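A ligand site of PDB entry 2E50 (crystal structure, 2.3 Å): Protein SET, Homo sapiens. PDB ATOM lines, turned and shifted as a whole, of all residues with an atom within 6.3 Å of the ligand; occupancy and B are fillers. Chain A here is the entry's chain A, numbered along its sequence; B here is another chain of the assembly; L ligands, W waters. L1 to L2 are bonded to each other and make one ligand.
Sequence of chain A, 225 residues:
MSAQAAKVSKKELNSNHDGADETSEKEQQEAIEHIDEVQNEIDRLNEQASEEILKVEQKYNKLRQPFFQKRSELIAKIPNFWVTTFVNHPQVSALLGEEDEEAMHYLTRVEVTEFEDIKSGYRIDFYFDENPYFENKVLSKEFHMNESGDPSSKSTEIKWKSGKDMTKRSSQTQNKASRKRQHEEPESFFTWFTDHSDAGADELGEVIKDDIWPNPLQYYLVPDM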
ATOM      1  N   GLU A  57     -15.628   1.949  18.137  1.00  0.00           N
ATOM      2  CA  GLU A  57     -16.652   2.785  18.773  1.00  0.00           C
ATOM      3  C   GLU A  57     -18.056   2.400  18.287  1.00  0.00           C
ATOM      4  O   GLU A  57     -18.982   2.338  19.087  1.00  0.00           O
ATOM      5  CB  GLU A  57     -16.364   4.269  18.490  1.00  0.00           C
ATOM      6  CG  GLU A  57     -17.438   5.274  18.962  1.00  0.00           C
ATOM      7  CD  GLU A  57     -17.442   5.478  20.467  1.00  0.00           C
ATOM      8  OE1 GLU A  57     -16.686   4.784  21.181  1.00  0.00           O
ATOM      9  OE2 GLU A  57     -18.224   6.309  20.966  1.00  0.00           O
ATOM     10  N   GLN A  58     -18.210   2.149  16.998  1.00  0.00           N
ATOM     11  CA  GLN A  58     -19.455   1.740  16.426  1.00  0.00           C
ATOM     12  C   GLN A  58     -19.856   0.405  17.027  1.00  0.00           C
ATOM     13  O   GLN A  58     -20.999   0.230  17.418  1.00  0.00           O
ATOM     14  CB  GLN A  58     -19.380   1.682  14.884  1.00  0.00           C
ATOM     15  CG  GLN A  58     -20.750   1.435  14.226  1.00  0.00           C
ATOM     16  CD  GLN A  58     -20.713   0.957  12.763  1.00  0.00           C
ATOM     17  OE1 GLN A  58     -19.652   0.577  12.228  1.00  0.00           O
ATOM     18  NE2 GLN A  58     -21.888   0.948  12.126  1.00  0.00           N
ATOM     19  N   TYR A  60     -19.112  -1.144  20.024  1.00  0.00           N
ATOM     20  CA  TYR A  60     -19.479  -1.061  21.429  1.00  0.00           C
ATOM     21  C   TYR A  60     -20.631  -0.109  21.673  1.00  0.00           C
ATOM     22  O   TYR A  60     -21.315  -0.200  22.694  1.00  0.00           O
ATOM     23  CB  TYR A  60     -18.256  -0.683  22.279  1.00  0.00           C
ATOM     24  CG  TYR A  60     -17.325  -1.895  22.409  1.00  0.00           C
ATOM     25  CD1 TYR A  60     -16.204  -2.050  21.562  1.00  0.00           C
ATOM     26  CD2 TYR A  60     -17.585  -2.882  23.328  1.00  0.00           C
ATOM     27  CE1 TYR A  60     -15.395  -3.165  21.681  1.00  0.00           C
ATOM     28  CE2 TYR A  60     -16.781  -4.001  23.455  1.00  0.00           C
ATOM     29  CZ  TYR A  60     -15.693  -4.142  22.648  1.00  0.00           C
ATOM     30  OH  TYR A  60     -14.909  -5.281  22.789  1.00  0.00           O
ATOM     31  N   ASN A  61     -20.873   0.786  20.730  1.00  0.00           N
ATOM     32  CA  ASN A  61     -21.993   1.677  20.862  1.00  0.00           C
ATOM     33  C   ASN A  61     -23.256   0.867  20.714  1.00  0.00           C
ATOM     34  O   ASN A  61     -24.195   1.084  21.461  1.00  0.00           O
ATOM     35  CB  ASN A  61     -21.891   2.807  19.845  1.00  0.00           C
ATOM     36  CG  ASN A  61     -21.178   4.009  20.409  1.00  0.00           C
ATOM     37  OD1 ASN A  61     -20.998   5.046  19.756  1.00  0.00           O
ATOM     38  ND2 ASN A  61     -20.771   3.879  21.680  1.00  0.00           N
ATOM     39  N   LYS A  62     -23.247  -0.036  19.722  1.00  0.00           N
ATOM     40  CA  LYS A  62     -24.344  -0.929  19.412  1.00  0.00           C
ATOM     41  C   LYS A  62     -24.569  -1.937  20.548  1.00  0.00           C
ATOM     42  O   LYS A  62     -25.686  -2.285  20.881  1.00  0.00           O
ATOM     43  CB  LYS A  62     -24.042  -1.686  18.091  1.00  0.00           C
ATOM     44  CG  LYS A  62     -24.445  -0.921  16.849  1.00  0.00           C
ATOM     45  CD  LYS A  62     -23.584  -1.331  15.599  1.00  0.00           C
ATOM     46  CE  LYS A  62     -24.081  -0.755  14.262  1.00  0.00           C
ATOM     47  NZ  LYS A  62     -23.577  -1.523  13.013  1.00  0.00           N
ATOM     48  N   ARG A  64     -23.773  -1.341  23.701  1.00  0.00           N
ATOM     49  CA  ARG A  64     -24.186  -0.587  24.858  1.00  0.00           C
ATOM     50  C   ARG A  64     -25.597  -0.114  24.805  1.00  0.00           C
ATOM     51  O   ARG A  64     -26.215  -0.062  25.826  1.00  0.00           O
ATOM     52  CB  ARG A  64     -23.257   0.611  25.136  1.00  0.00           C
ATOM     53  CG  ARG A  64     -21.971   0.132  25.786  1.00  0.00           C
ATOM     54  CD  ARG A  64     -20.915   1.241  25.954  1.00  0.00           C
ATOM     55  NE  ARG A  64     -20.349   1.697  24.720  1.00  0.00           N
ATOM     56  CZ  ARG A  64     -19.270   2.513  24.623  1.00  0.00           C
ATOM     57  NH1 ARG A  64     -18.633   2.952  25.707  1.00  0.00           N
ATOM     58  NH2 ARG A  64     -18.839   2.875  23.449  1.00  0.00           N
ATOM     59  N   GLN A  65     -26.076   0.263  23.630  1.00  0.00           N
ATOM     60  CA  GLN A  65     -27.350   0.888  23.512  1.00  0.00           C
ATOM     61  C   GLN A  65     -28.540   0.192  24.242  1.00  0.00           C
ATOM     62  O   GLN A  65     -29.216   0.815  25.043  1.00  0.00           O
ATOM     63  CB  GLN A  65     -27.635   1.140  22.043  1.00  0.00           C
ATOM     64  CG  GLN A  65     -28.932   1.893  21.814  1.00  0.00           C
ATOM     65  CD  GLN A  65     -29.168   2.173  20.360  1.00  0.00           C
ATOM     66  OE1 GLN A  65     -28.783   1.366  19.492  1.00  0.00           O
ATOM     67  NE2 GLN A  65     -29.773   3.314  20.064  1.00  0.00           N
ATOM     68  N   PRO A  66     -28.771  -1.118  23.990  1.00  0.00           N
ATOM     69  CA  PRO A  66     -29.910  -1.791  24.661  1.00  0.00           C
ATOM     70  C   PRO A  66     -29.815  -1.720  26.178  1.00  0.00           C
ATOM     71  O   PRO A  66     -30.843  -1.608  26.857  1.00  0.00           O
ATOM     72  CB  PRO A  66     -29.820  -3.239  24.213  1.00  0.00           C
ATOM     73  CG  PRO A  66     -28.781  -3.284  23.124  1.00  0.00           C
ATOM     74  CD  PRO A  66     -28.028  -2.019  23.083  1.00  0.00           C
ATOM     75  N   PHE A  68     -28.359   0.842  27.959  1.00  0.00           N
ATOM     76  CA  PHE A  68     -28.714   2.217  28.390  1.00  0.00           C
ATOM     77  C   PHE A  68     -30.199   2.421  28.251  1.00  0.00           C
ATOM     78  O   PHE A  68     -30.781   3.044  29.129  1.00  0.00           O
ATOM     79  CB  PHE A  68     -27.968   3.314  27.592  1.00  0.00           C
ATOM     80  CG  PHE A  68     -26.550   3.533  27.999  1.00  0.00           C
ATOM     81  CD1 PHE A  68     -25.531   2.645  27.629  1.00  0.00           C
ATOM     82  CD2 PHE A  68     -26.218   4.633  28.776  1.00  0.00           C
ATOM     83  CE1 PHE A  68     -24.166   2.890  27.993  1.00  0.00           C
ATOM     84  CE2 PHE A  68     -24.887   4.908  29.147  1.00  0.00           C
ATOM     85  CZ  PHE A  68     -23.843   4.028  28.759  1.00  0.00           C
ATOM     86  N   GLN A  69     -30.817   1.945  27.158  1.00  0.00           N
ATOM     87  CA  GLN A  69     -32.332   1.848  27.079  1.00  0.00           C
ATOM     88  C   GLN A  69     -33.002   1.127  28.247  1.00  0.00           C
ATOM     89  O   GLN A  69     -33.925   1.650  28.884  1.00  0.00           O
ATOM     90  CB  GLN A  69     -32.818   1.222  25.771  1.00  0.00           C
ATOM     91  CG  GLN A  69     -32.312   1.973  24.559  1.00  0.00           C
ATOM     92  CD  GLN A  69     -32.644   1.264  23.266  1.00  0.00           C
ATOM     93  OE1 GLN A  69     -32.868   0.055  23.271  1.00  0.00           O
ATOM     94  NE2 GLN A  69     -32.612   2.002  22.147  1.00  0.00           N
ATOM     95  N   ARG A  71     -31.670   0.652  31.152  1.00  0.00           N
ATOM     96  CA  ARG A  71     -31.355   1.403  32.370  1.00  0.00           C
ATOM     97  C   ARG A  71     -32.289   2.583  32.592  1.00  0.00           C
ATOM     98  O   ARG A  71     -32.783   2.796  33.715  1.00  0.00           O
ATOM     99  CB  ARG A  71     -29.887   1.883  32.364  1.00  0.00           C
ATOM    100  CG  ARG A  71     -29.425   2.416  33.710  1.00  0.00           C
ATOM    101  CD  ARG A  71     -28.064   3.072  33.597  1.00  0.00           C
ATOM    102  NE  ARG A  71     -28.112   4.366  32.892  1.00  0.00           N
ATOM    103  CZ  ARG A  71     -27.026   5.065  32.538  1.00  0.00           C
ATOM    104  NH1 ARG A  71     -25.816   4.590  32.770  1.00  0.00           N
ATOM    105  NH2 ARG A  71     -27.156   6.205  31.884  1.00  0.00           N
ATOM    106  N   GLU A 111     -32.314  11.878  29.577  1.00  0.00           N
ATOM    107  CA  GLU A 111     -31.644  11.251  28.423  1.00  0.00           C
ATOM    108  C   GLU A 111     -30.534  12.121  27.910  1.00  0.00           C
ATOM    109  O   GLU A 111     -30.767  13.253  27.612  1.00  0.00           O
ATOM    110  CB  GLU A 111     -32.599  11.062  27.249  1.00  0.00           C
ATOM    111  CG  GLU A 111     -33.364   9.808  27.186  1.00  0.00           C
ATOM    112  CD  GLU A 111     -32.530   8.543  27.346  1.00  0.00           C
ATOM    113  OE1 GLU A 111     -32.820   7.937  28.381  1.00  0.00           O
ATOM    114  OE2 GLU A 111     -31.704   8.106  26.469  1.00  0.00           O
ATOM    115  N   VAL A 112     -29.343  11.564  27.788  1.00  0.00           N
ATOM    116  CA  VAL A 112     -28.249  12.196  27.039  1.00  0.00           C
ATOM    117  C   VAL A 112     -28.106  11.432  25.699  1.00  0.00           C
ATOM    118  O   VAL A 112     -27.961  10.217  25.715  1.00  0.00           O
ATOM    119  CB  VAL A 112     -26.910  12.204  27.795  1.00  0.00           C
ATOM    120  CG1 VAL A 112     -25.851  12.933  27.008  1.00  0.00           C
ATOM    121  CG2 VAL A 112     -27.080  12.810  29.201  1.00  0.00           C
ATOM    122  N   THR A 113     -28.157  12.157  24.576  1.00  0.00           N
ATOM    123  CA  THR A 113     -28.024  11.579  23.243  1.00  0.00           C
ATOM    124  C   THR A 113     -26.971  12.401  22.553  1.00  0.00           C
ATOM    125  O   THR A 113     -27.067  13.610  22.529  1.00  0.00           O
ATOM    126  CB  THR A 113     -29.358  11.693  22.453  1.00  0.00           C
ATOM    127  OG1 THR A 113     -30.449  11.276  23.281  1.00  0.00           O
ATOM    128  CG2 THR A 113     -29.341  10.872  21.174  1.00  0.00           C
ATOM    129  N   GLU A 114     -25.945  11.732  22.052  1.00  0.00           N
ATOM    130  CA  GLU A 114     -24.831  12.301  21.338  1.00  0.00           C
ATOM    131  C   GLU A 114     -25.022  11.939  19.876  1.00  0.00           C
ATOM    132  O   GLU A 114     -25.391  10.811  19.569  1.00  0.00           O
ATOM    133  CB  GLU A 114     -23.468  11.774  21.878  1.00  0.00           C
ATOM    134  CG  GLU A 114     -23.354  11.986  23.413  1.00  0.00           C
ATOM    135  CD  GLU A 114     -22.230  11.194  24.151  1.00  0.00           C
ATOM    136  OE1 GLU A 114     -22.515  10.615  25.278  1.00  0.00           O
ATOM    137  OE2 GLU A 114     -21.084  11.199  23.611  1.00  0.00           O
ATOM    138  N   PHE A 115     -24.789  12.895  18.972  1.00  0.00           N
ATOM    139  CA  PHE A 115     -24.972  12.665  17.543  1.00  0.00           C
ATOM    140  C   PHE A 115     -23.685  12.539  16.764  1.00  0.00           C
ATOM    141  O   PHE A 115     -23.755  12.457  15.534  1.00  0.00           O
ATOM    142  CB  PHE A 115     -25.852  13.769  16.942  1.00  0.00           C
ATOM    143  CG  PHE A 115     -27.056  14.080  17.776  1.00  0.00           C
ATOM    144  CD1 PHE A 115     -27.088  15.202  18.584  1.00  0.00           C
ATOM    145  CD2 PHE A 115     -28.125  13.203  17.815  1.00  0.00           C
ATOM    146  CE1 PHE A 115     -28.197  15.457  19.375  1.00  0.00           C
ATOM    147  CE2 PHE A 115     -29.209  13.466  18.588  1.00  0.00           C
ATOM    148  CZ  PHE A 115     -29.251  14.568  19.390  1.00  0.00           C
ATOM    149  N   GLU A 116     -22.529  12.504  17.443  1.00  0.00           N
ATOM    150  CA  GLU A 116     -21.185  12.754  16.804  1.00  0.00           C
ATOM    151  C   GLU A 116     -21.055  12.552  15.303  1.00  0.00           C
ATOM    152  O   GLU A 116     -20.614  13.463  14.584  1.00  0.00           O
ATOM    153  CB  GLU A 116     -20.053  11.979  17.488  1.00  0.00           C
ATOM    154  CG  GLU A 116     -19.103  12.787  18.385  1.00  0.00           C
ATOM    155  CD  GLU A 116     -17.881  11.949  18.815  1.00  0.00           C
ATOM    156  OE1 GLU A 116     -17.897  11.388  19.958  1.00  0.00           O
ATOM    157  OE2 GLU A 116     -16.922  11.825  17.984  1.00  0.00           O
ATOM    158  N   TRP A 213     -23.757  10.431  33.098  1.00  0.00           N
ATOM    159  CA  TRP A 213     -24.439   9.537  32.150  1.00  0.00           C
ATOM    160  C   TRP A 213     -23.881   8.109  32.026  1.00  0.00           C
ATOM    161  O   TRP A 213     -24.664   7.177  32.050  1.00  0.00           O
ATOM    162  CB  TRP A 213     -24.556  10.166  30.768  1.00  0.00           C
ATOM    163  CG  TRP A 213     -25.461   9.406  29.895  1.00  0.00           C
ATOM    164  CD1 TRP A 213     -25.120   8.693  28.792  1.00  0.00           C
ATOM    165  CD2 TRP A 213     -26.872   9.228  30.080  1.00  0.00           C
ATOM    166  NE1 TRP A 213     -26.214   8.118  28.268  1.00  0.00           N
ATOM    167  CE2 TRP A 213     -27.306   8.420  29.030  1.00  0.00           C
ATOM    168  CE3 TRP A 213     -27.799   9.685  31.046  1.00  0.00           C
ATOM    169  CZ2 TRP A 213     -28.646   8.027  28.893  1.00  0.00           C
ATOM    170  CZ3 TRP A 213     -29.127   9.318  30.891  1.00  0.00           C
ATOM    171  CH2 TRP A 213     -29.534   8.474  29.842  1.00  0.00           C
ATOM    172  N   PRO A 214     -22.544   7.921  31.852  1.00  0.00           N
ATOM    173  CA  PRO A 214     -22.040   6.553  31.707  1.00  0.00           C
ATOM    174  C   PRO A 214     -22.338   5.630  32.909  1.00  0.00           C
ATOM    175  O   PRO A 214     -22.389   4.417  32.736  1.00  0.00           O
ATOM    176  CB  PRO A 214     -20.493   6.731  31.619  1.00  0.00           C
ATOM    177  CG  PRO A 214     -20.293   8.171  31.150  1.00  0.00           C
ATOM    178  CD  PRO A 214     -21.455   8.928  31.781  1.00  0.00           C
ATOM    179  N   ASN B  46     -17.922  -0.435  28.672  1.00  0.00           N
ATOM    180  CA  ASN B  46     -17.105   0.790  28.688  1.00  0.00           C
ATOM    181  C   ASN B  46     -15.632   0.441  28.812  1.00  0.00           C
ATOM    182  O   ASN B  46     -14.811   1.001  28.126  1.00  0.00           O
ATOM    183  CB  ASN B  46     -17.485   1.718  29.852  1.00  0.00           C
ATOM    184  CG  ASN B  46     -18.803   2.443  29.631  1.00  0.00           C
ATOM    185  OD1 ASN B  46     -19.308   2.528  28.523  1.00  0.00           O
ATOM    186  ND2 ASN B  46     -19.350   2.994  30.708  1.00  0.00           N
HETATM  187  C1  LIG L   1     -24.965   4.483  22.924  1.00  0.00           C
HETATM  188  C2  LIG L   1     -26.066   4.611  23.985  1.00  0.00           C
HETATM  189  C3  LIG L   1     -25.848   5.872  24.799  1.00  0.00           C
HETATM  190  C4  LIG L   1     -24.496   5.792  25.482  1.00  0.00           C
HETATM  191  C5  LIG L   1     -23.426   5.686  24.437  1.00  0.00           C
HETATM  192  C6  LIG L   1     -22.006   5.693  25.028  1.00  0.00           C
HETATM  193  O1  LIG L   1     -27.378   4.622  23.494  1.00  0.00           O
HETATM  194  O2  LIG L   1     -26.900   6.054  25.734  1.00  0.00           O
HETATM  195  O3  LIG L   1     -24.219   6.963  26.257  1.00  0.00           O
HETATM  196  O4  LIG L   1     -23.686   4.545  23.607  1.00  0.00           O
HETATM  197  O5  LIG L   1     -21.237   4.942  24.079  1.00  0.00           O
HETATM  198  C1  LG2 L   2     -24.192   5.564  20.974  1.00  0.00           C
HETATM  199  C2  LG2 L   2     -24.201   6.899  20.210  1.00  0.00           C
HETATM  200  C3  LG2 L   2     -25.533   7.125  19.493  1.00  0.00           C
HETATM  201  C4  LG2 L   2     -25.867   5.920  18.620  1.00  0.00           C
HETATM  202  C5  LG2 L   2     -25.996   4.745  19.572  1.00  0.00           C
HETATM  203  C6  LG2 L   2     -26.393   3.509  18.772  1.00  0.00           C
HETATM  204  O1  LG2 L   2     -25.019   5.658  22.110  1.00  0.00           O
HETATM  205  O2  LG2 L   2     -23.899   7.932  21.136  1.00  0.00           O
HETATM  206  O3  LG2 L   2     -25.493   8.299  18.726  1.00  0.00           O
HETATM  207  O4  LG2 L   2     -27.170   5.999  18.063  1.00  0.00           O
HETATM  208  O5  LG2 L   2     -24.741   4.499  20.229  1.00  0.00           O
HETATM  209  O6  LG2 L   2     -25.252   3.308  17.955  1.00  0.00           O
HETATM  210  O   HOH W   1     -22.524   4.535  16.979  1.00  0.00           O
HETATM  211  O   HOH W   2     -22.186   7.169  27.951  1.00  0.00           O
HETATM  212  O   HOH W   3     -28.877   7.939  25.042  1.00  0.00           O
HETATM  213  O   HOH W   4     -28.097   7.253  22.289  1.00  0.00           O
HETATM  214  O   HOH W   5     -29.136   6.824  19.947  1.00  0.00           O
HETATM  215  O   HOH W   6     -25.255   9.397  25.086  1.00  0.00           O
HETATM  216  O   HOH W   7     -30.036   4.322  24.765  1.00  0.00           O
HETATM  217  O   HOH W   8     -25.923   8.718  22.647  1.00  0.00           O
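Gln 65 touches the ligand.
CG of Phe 68 touches O2 of LIG L1, at 3.4 Å.
The nearest printed residue that does not touch the ligand is Lys 62 (4.3 Å).
The guanidinium group (NH2) of Arg 64 sits close to the side-chain amide nitrogen (ND2) of Asn 61 (2.8 Å).
The side-chain carboxylate (OE2) of Glu 57 sits close to the side-chain amide oxygen (OD1) of Asn 61 (3.3 Å).
The backbone carbonyl oxygen (O) of Trp 213 is in hydrogen-bond range of the guanidinium group (NH2) of Arg 71.
NH2 of Arg 64 is in salt-bridge range of OE1 of Glu 57 (3.7 Å).
O of Tyr 60 sits at hydrogen-bond distance from NE of Arg 64, at 2.9 Å.
NH1 of Arg 64 sits at hydrogen-bond distance from OD1 of Asn 46 of chain B.
Water W8 bridges O2 of LG2 L2 (2.6 Å) and N of Glu 114 (3.1 Å).
Water W3 lies within hydrogen-bond range of the backbone carbonyl oxygen of Val 112 (2.5 Å), an oxygen (O2) of LIG L1 (2.8 Å) and the side-chain carboxylate of Glu 111 (3.2 Å).
Water W6 lies within hydrogen-bond range of an oxygen (O3) of LIG L1 (2.9 Å), the backbone carbonyl oxygen of Val 112 (2.9 Å) and the side-chain carboxylate of Glu 114 (3.0 Å).
Water W7 bridges O1 of LIG L1 (3.0 Å) and N of Gln 69 (3.5 Å).
Water W1 lies within hydrogen-bond range of an oxygen (O6) of LG2 L2 and the side-chain amide oxygen of Asn 61.
The backbone carbonyl oxygen of Glu 114 sits at hydrogen-bond distance from an oxygen (O3) of LG2 L2 (2.7 Å).
ND2 of Asn 61 is in hydrogen-bond range of O5 of LIG L1, 2.7 Å away.
O3 of LIG L1 is in hydrogen-bond range of NE1 of Trp 213, 3.1 Å away.
The guanidinium group (NH2) of Arg 64 lies close to an oxygen (O5) of LIG L1, 3.2 Å away.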
